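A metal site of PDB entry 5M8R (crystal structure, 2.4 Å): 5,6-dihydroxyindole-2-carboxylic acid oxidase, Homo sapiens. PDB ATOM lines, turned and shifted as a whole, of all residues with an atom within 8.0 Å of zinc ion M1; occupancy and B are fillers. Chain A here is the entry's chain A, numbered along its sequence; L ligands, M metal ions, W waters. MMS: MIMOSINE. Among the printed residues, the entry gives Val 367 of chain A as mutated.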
ATOM      1  N   HIS A 168      32.090 -20.990  -0.027  1.00  0.00           N
ATOM      2  CA  HIS A 168      31.030 -21.749   0.623  1.00  0.00           C
ATOM      3  C   HIS A 168      29.681 -21.497  -0.049  1.00  0.00           C
ATOM      4  O   HIS A 168      28.897 -22.439  -0.249  1.00  0.00           O
ATOM      5  CB  HIS A 168      30.976 -21.372   2.119  1.00  0.00           C
ATOM      6  CG  HIS A 168      30.190 -22.318   2.980  1.00  0.00           C
ATOM      7  ND1 HIS A 168      28.896 -22.067   3.383  1.00  0.00           N
ATOM      8  CD2 HIS A 168      30.537 -23.487   3.576  1.00  0.00           C
ATOM      9  CE1 HIS A 168      28.466 -23.060   4.148  1.00  0.00           C
ATOM     10  NE2 HIS A 168      29.445 -23.931   4.290  1.00  0.00           N
ATOM     11  N   SER A 190      29.097 -29.402  -0.795  1.00  0.00           N
ATOM     12  CA  SER A 190      29.884 -29.396   0.426  1.00  0.00           C
ATOM     13  C   SER A 190      29.139 -29.860   1.673  1.00  0.00           C
ATOM     14  O   SER A 190      29.745 -29.891   2.743  1.00  0.00           O
ATOM     15  CB  SER A 190      30.429 -27.992   0.692  1.00  0.00           C
ATOM     16  OG  SER A 190      29.351 -27.066   0.729  1.00  0.00           O
ATOM     17  N   HIS A 191      27.860 -30.236   1.555  1.00  0.00           N
ATOM     18  CA  HIS A 191      27.076 -30.722   2.681  1.00  0.00           C
ATOM     19  C   HIS A 191      26.231 -31.887   2.225  1.00  0.00           C
ATOM     20  O   HIS A 191      26.100 -32.153   1.031  1.00  0.00           O
ATOM     21  CB  HIS A 191      26.160 -29.632   3.265  1.00  0.00           C
ATOM     22  CG  HIS A 191      26.868 -28.358   3.532  1.00  0.00           C
ATOM     23  ND1 HIS A 191      27.269 -27.491   2.535  1.00  0.00           N
ATOM     24  CD2 HIS A 191      27.307 -27.818   4.696  1.00  0.00           C
ATOM     25  CE1 HIS A 191      27.898 -26.471   3.074  1.00  0.00           C
ATOM     26  NE2 HIS A 191      27.929 -26.632   4.379  1.00  0.00           N
ATOM     27  N   PHE A 196      31.597 -33.530   3.032  1.00  0.00           N
ATOM     28  CA  PHE A 196      31.330 -32.457   3.987  1.00  0.00           C
ATOM     29  C   PHE A 196      32.574 -32.125   4.820  1.00  0.00           C
ATOM     30  O   PHE A 196      32.948 -30.955   4.967  1.00  0.00           O
ATOM     31  CB  PHE A 196      30.160 -32.848   4.901  1.00  0.00           C
ATOM     32  CG  PHE A 196      30.076 -32.017   6.165  1.00  0.00           C
ATOM     33  CD1 PHE A 196      29.599 -30.715   6.135  1.00  0.00           C
ATOM     34  CD2 PHE A 196      30.490 -32.547   7.387  1.00  0.00           C
ATOM     35  CE1 PHE A 196      29.547 -29.949   7.299  1.00  0.00           C
ATOM     36  CE2 PHE A 196      30.435 -31.788   8.539  1.00  0.00           C
ATOM     37  CZ  PHE A 196      29.961 -30.495   8.504  1.00  0.00           C
ATOM     38  N   HIS A 200      35.189 -28.865   4.142  1.00  0.00           N
ATOM     39  CA  HIS A 200      35.342 -27.811   5.154  1.00  0.00           C
ATOM     40  C   HIS A 200      36.745 -27.793   5.724  1.00  0.00           C
ATOM     41  O   HIS A 200      37.201 -26.736   6.158  1.00  0.00           O
ATOM     42  CB  HIS A 200      34.298 -27.969   6.262  1.00  0.00           C
ATOM     43  CG  HIS A 200      32.924 -27.527   5.842  1.00  0.00           C
ATOM     44  ND1 HIS A 200      32.095 -28.305   5.068  1.00  0.00           N
ATOM     45  CD2 HIS A 200      32.262 -26.352   6.038  1.00  0.00           C
ATOM     46  CE1 HIS A 200      30.976 -27.651   4.823  1.00  0.00           C
ATOM     47  NE2 HIS A 200      31.043 -26.471   5.411  1.00  0.00           N
ATOM     48  N   HIS A 203      38.700 -25.681   3.202  1.00  0.00           N
ATOM     49  CA  HIS A 203      38.161 -24.354   3.454  1.00  0.00           C
ATOM     50  C   HIS A 203      38.907 -23.650   4.587  1.00  0.00           C
ATOM     51  O   HIS A 203      39.416 -22.530   4.418  1.00  0.00           O
ATOM     52  CB  HIS A 203      36.674 -24.508   3.793  1.00  0.00           C
ATOM     53  CG  HIS A 203      35.874 -23.252   3.697  1.00  0.00           C
ATOM     54  ND1 HIS A 203      34.796 -23.002   4.525  1.00  0.00           N
ATOM     55  CD2 HIS A 203      35.946 -22.197   2.845  1.00  0.00           C
ATOM     56  CE1 HIS A 203      34.267 -21.833   4.213  1.00  0.00           C
ATOM     57  NE2 HIS A 203      34.937 -21.329   3.192  1.00  0.00           N
ATOM     58  N   GLU A 336      28.254 -34.351  11.168  1.00  0.00           N
ATOM     59  CA  GLU A 336      27.601 -33.279  10.437  1.00  0.00           C
ATOM     60  C   GLU A 336      26.312 -32.871  11.130  1.00  0.00           C
ATOM     61  O   GLU A 336      25.990 -31.682  11.198  1.00  0.00           O
ATOM     62  CB  GLU A 336      27.333 -33.673   8.978  1.00  0.00           C
ATOM     63  CG  GLU A 336      26.706 -32.492   8.223  1.00  0.00           C
ATOM     64  CD  GLU A 336      26.535 -32.699   6.736  1.00  0.00           C
ATOM     65  OE1 GLU A 336      26.897 -33.774   6.229  1.00  0.00           O
ATOM     66  OE2 GLU A 336      26.037 -31.749   6.076  1.00  0.00           O
ATOM     67  N   HIS A 353      27.333 -30.610  14.713  1.00  0.00           N
ATOM     68  CA  HIS A 353      27.674 -29.445  13.877  1.00  0.00           C
ATOM     69  C   HIS A 353      26.436 -28.695  13.394  1.00  0.00           C
ATOM     70  O   HIS A 353      26.407 -27.464  13.400  1.00  0.00           O
ATOM     71  CB  HIS A 353      28.537 -29.899  12.694  1.00  0.00           C
ATOM     72  CG  HIS A 353      28.385 -29.055  11.467  1.00  0.00           C
ATOM     73  ND1 HIS A 353      27.472 -29.337  10.478  1.00  0.00           N
ATOM     74  CD2 HIS A 353      29.029 -27.929  11.077  1.00  0.00           C
ATOM     75  CE1 HIS A 353      27.553 -28.429   9.524  1.00  0.00           C
ATOM     76  NE2 HIS A 353      28.503 -27.555   9.861  1.00  0.00           N
ATOM     77  N   ASN A 354      25.403 -29.421  12.948  1.00  0.00           N
ATOM     78  CA  ASN A 354      24.168 -28.753  12.550  1.00  0.00           C
ATOM     79  C   ASN A 354      23.553 -27.990  13.726  1.00  0.00           C
ATOM     80  O   ASN A 354      23.100 -26.848  13.563  1.00  0.00           O
ATOM     81  CB  ASN A 354      23.170 -29.769  11.998  1.00  0.00           C
ATOM     82  CG  ASN A 354      23.494 -30.219  10.589  1.00  0.00           C
ATOM     83  OD1 ASN A 354      24.228 -29.557   9.855  1.00  0.00           O
ATOM     84  ND2 ASN A 354      22.910 -31.328  10.177  1.00  0.00           N
ATOM     85  N   ALA A 356      24.975 -26.722  16.460  1.00  0.00           N
ATOM     86  CA  ALA A 356      25.704 -25.499  16.770  1.00  0.00           C
ATOM     87  C   ALA A 356      25.315 -24.376  15.809  1.00  0.00           C
ATOM     88  O   ALA A 356      25.219 -23.211  16.217  1.00  0.00           O
ATOM     89  CB  ALA A 356      27.206 -25.760  16.756  1.00  0.00           C
ATOM     90  N   HIS A 357      25.065 -24.710  14.540  1.00  0.00           N
ATOM     91  CA  HIS A 357      24.656 -23.683  13.586  1.00  0.00           C
ATOM     92  C   HIS A 357      23.298 -23.118  13.942  1.00  0.00           C
ATOM     93  O   HIS A 357      23.098 -21.894  13.948  1.00  0.00           O
ATOM     94  CB  HIS A 357      24.585 -24.253  12.173  1.00  0.00           C
ATOM     95  CG  HIS A 357      25.866 -24.215  11.411  1.00  0.00           C
ATOM     96  ND1 HIS A 357      26.361 -23.057  10.832  1.00  0.00           N
ATOM     97  CD2 HIS A 357      26.745 -25.193  11.080  1.00  0.00           C
ATOM     98  CE1 HIS A 357      27.486 -23.332  10.196  1.00  0.00           C
ATOM     99  NE2 HIS A 357      27.735 -24.614  10.332  1.00  0.00           N
ATOM    100  N   GLY A 364      24.486 -17.198  11.042  1.00  0.00           N
ATOM    101  CA  GLY A 364      25.226 -18.456  11.141  1.00  0.00           C
ATOM    102  C   GLY A 364      24.385 -19.714  11.012  1.00  0.00           C
ATOM    103  O   GLY A 364      24.953 -20.820  10.906  1.00  0.00           O
ATOM    104  N   VAL A 367      22.748 -21.869   5.534  1.00  0.00           N
ATOM    105  CA  VAL A 367      23.930 -22.523   4.945  1.00  0.00           C
ATOM    106  C   VAL A 367      24.569 -21.663   3.848  1.00  0.00           C
ATOM    107  O   VAL A 367      25.790 -21.671   3.697  1.00  0.00           O
ATOM    108  CB  VAL A 367      23.557 -23.942   4.460  1.00  0.00           C
ATOM    109  CG1 VAL A 367      22.674 -23.896   3.272  1.00  0.00           C
ATOM    110  CG2 VAL A 367      24.813 -24.778   4.169  1.00  0.00           C
ATOM    111  N   SER A 370      26.271 -18.699   6.298  1.00  0.00           N
ATOM    112  CA  SER A 370      26.759 -18.851   7.656  1.00  0.00           C
ATOM    113  C   SER A 370      28.236 -18.468   7.861  1.00  0.00           C
ATOM    114  O   SER A 370      28.536 -17.983   8.957  1.00  0.00           O
ATOM    115  CB  SER A 370      26.448 -20.274   8.125  1.00  0.00           C
ATOM    116  OG  SER A 370      27.065 -21.245   7.303  1.00  0.00           O
ATOM    117  N   PRO A 371      29.151 -18.564   6.877  1.00  0.00           N
ATOM    118  CA  PRO A 371      30.517 -18.052   7.140  1.00  0.00           C
ATOM    119  C   PRO A 371      30.565 -16.558   7.407  1.00  0.00           C
ATOM    120  O   PRO A 371      31.595 -16.088   7.919  1.00  0.00           O
ATOM    121  CB  PRO A 371      31.298 -18.387   5.857  1.00  0.00           C
ATOM    122  CG  PRO A 371      30.505 -19.449   5.163  1.00  0.00           C
ATOM    123  CD  PRO A 371      29.072 -19.178   5.538  1.00  0.00           C
ATOM    124  N   PHE A 376      31.648 -19.206  12.568  1.00  0.00           N
ATOM    125  CA  PHE A 376      31.767 -20.311  11.630  1.00  0.00           C
ATOM    126  C   PHE A 376      33.174 -20.925  11.661  1.00  0.00           C
ATOM    127  O   PHE A 376      33.324 -22.156  11.719  1.00  0.00           O
ATOM    128  CB  PHE A 376      31.414 -19.792  10.231  1.00  0.00           C
ATOM    129  CG  PHE A 376      31.487 -20.841   9.133  1.00  0.00           C
ATOM    130  CD1 PHE A 376      32.694 -21.180   8.562  1.00  0.00           C
ATOM    131  CD2 PHE A 376      30.333 -21.448   8.670  1.00  0.00           C
ATOM    132  CE1 PHE A 376      32.771 -22.115   7.548  1.00  0.00           C
ATOM    133  CE2 PHE A 376      30.393 -22.380   7.659  1.00  0.00           C
ATOM    134  CZ  PHE A 376      31.624 -22.723   7.092  1.00  0.00           C
ATOM    135  N   LEU A 379      33.580 -22.829  14.954  1.00  0.00           N
ATOM    136  CA  LEU A 379      32.672 -23.967  14.909  1.00  0.00           C
ATOM    137  C   LEU A 379      33.211 -25.079  14.003  1.00  0.00           C
ATOM    138  O   LEU A 379      33.066 -26.273  14.307  1.00  0.00           O
ATOM    139  CB  LEU A 379      31.294 -23.470  14.431  1.00  0.00           C
ATOM    140  CG  LEU A 379      30.045 -24.341  14.355  1.00  0.00           C
ATOM    141  CD1 LEU A 379      28.859 -23.415  14.073  1.00  0.00           C
ATOM    142  CD2 LEU A 379      30.140 -25.388  13.250  1.00  0.00           C
ATOM    143  N   HIS A 380      33.853 -24.706  12.891  1.00  0.00           N
ATOM    144  CA  HIS A 380      34.388 -25.717  11.974  1.00  0.00           C
ATOM    145  C   HIS A 380      35.803 -26.182  12.290  1.00  0.00           C
ATOM    146  O   HIS A 380      36.128 -27.323  11.984  1.00  0.00           O
ATOM    147  CB  HIS A 380      34.333 -25.220  10.527  1.00  0.00           C
ATOM    148  CG  HIS A 380      33.093 -25.674   9.830  1.00  0.00           C
ATOM    149  ND1 HIS A 380      32.905 -26.974   9.419  1.00  0.00           N
ATOM    150  CD2 HIS A 380      31.930 -25.025   9.585  1.00  0.00           C
ATOM    151  CE1 HIS A 380      31.696 -27.101   8.922  1.00  0.00           C
ATOM    152  NE2 HIS A 380      31.087 -25.932   8.992  1.00  0.00           N
ATOM    153  N   THR A 383      34.792 -28.963  14.518  1.00  0.00           N
ATOM    154  CA  THR A 383      34.342 -30.097  13.723  1.00  0.00           C
ATOM    155  C   THR A 383      35.509 -30.790  13.042  1.00  0.00           C
ATOM    156  O   THR A 383      35.536 -32.021  12.924  1.00  0.00           O
ATOM    157  CB  THR A 383      33.334 -29.640  12.664  1.00  0.00           C
ATOM    158  OG1 THR A 383      32.253 -28.912  13.278  1.00  0.00           O
ATOM    159  CG2 THR A 383      32.792 -30.846  11.910  1.00  0.00           C
HETATM  160  O4  MMS L   1      26.318 -26.543   7.484  1.00  0.00           O
HETATM  161  C1  MMS L   1      20.118 -28.395   9.078  1.00  0.00           C
HETATM  162  O1  MMS L   1      20.166 -28.792  10.275  1.00  0.00           O
HETATM  163  O2  MMS L   1      19.053 -28.514   8.409  1.00  0.00           O
HETATM  164  N1  MMS L   1      20.996 -27.242   7.096  1.00  0.00           N
HETATM  165  C2  MMS L   1      21.341 -27.758   8.417  1.00  0.00           C
HETATM  166  C3  MMS L   1      21.787 -26.629   9.329  1.00  0.00           C
HETATM  167  N2  MMS L   1      22.916 -25.897   8.820  1.00  0.00           N
HETATM  168  C8  MMS L   1      24.133 -26.613   8.371  1.00  0.00           C
HETATM  169  C4  MMS L   1      22.856 -24.403   8.767  1.00  0.00           C
HETATM  170  C7  MMS L   1      25.155 -25.913   7.909  1.00  0.00           C
HETATM  171  C5  MMS L   1      23.885 -23.703   8.311  1.00  0.00           C
HETATM  172  C6  MMS L   1      25.125 -24.418   7.853  1.00  0.00           C
HETATM  173  O3  MMS L   1      26.076 -23.836   7.446  1.00  0.00           O
HETATM  174 ZN    ZN M   1      28.952 -25.711   9.012  1.00  0.00          ZN
HETATM  175 ZN    ZN M   2      29.275 -25.535   5.477  1.00  0.00          ZN
HETATM  176  O   HOH W   1      28.278 -25.055   7.242  1.00  0.00           O
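A ring nitrogen (NE2) of His 191 lies close to an oxygen (O4) of the ligand, at 3.5 Å.
NE2 of His 353 sits close to O4 of the ligand (3.4 Å).
An oxygen (O3) of the ligand is in hydrogen-bond range of the side-chain hydroxyl (OG) of Ser 370 (2.8 Å).
An oxygen (O3) of the ligand sits close to a ring nitrogen (ND1) of His 357 (3.5 Å).
The backbone carbonyl oxygen (O) of Gly 364 lies within hydrogen-bond range of a ring nitrogen (ND1) of His 357.
ND1 of His 353 sits at hydrogen-bond distance from O of Glu 336, 2.9 Å away.
ND1 of His 353 is in hydrogen-bond range of OD1 of Asn 354 (3.3 Å).
Phe 376 touches zinc ion M1.
Of the 19 residues printed, 4 come within 4 Å of zinc ion M1.
The nearest printed residue that does not touch zinc ion M1 is His 200 (4.2 Å).
Zinc ion M1 is bound by water W1.
NE2 of His 353 binds zinc ion M1, at 2.1 Å.
Zinc ion M1 is bound by NE2 of His 357 (2.1 Å).
Zinc ion M1 is bound by NE2 of His 380 (2.1 Å).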
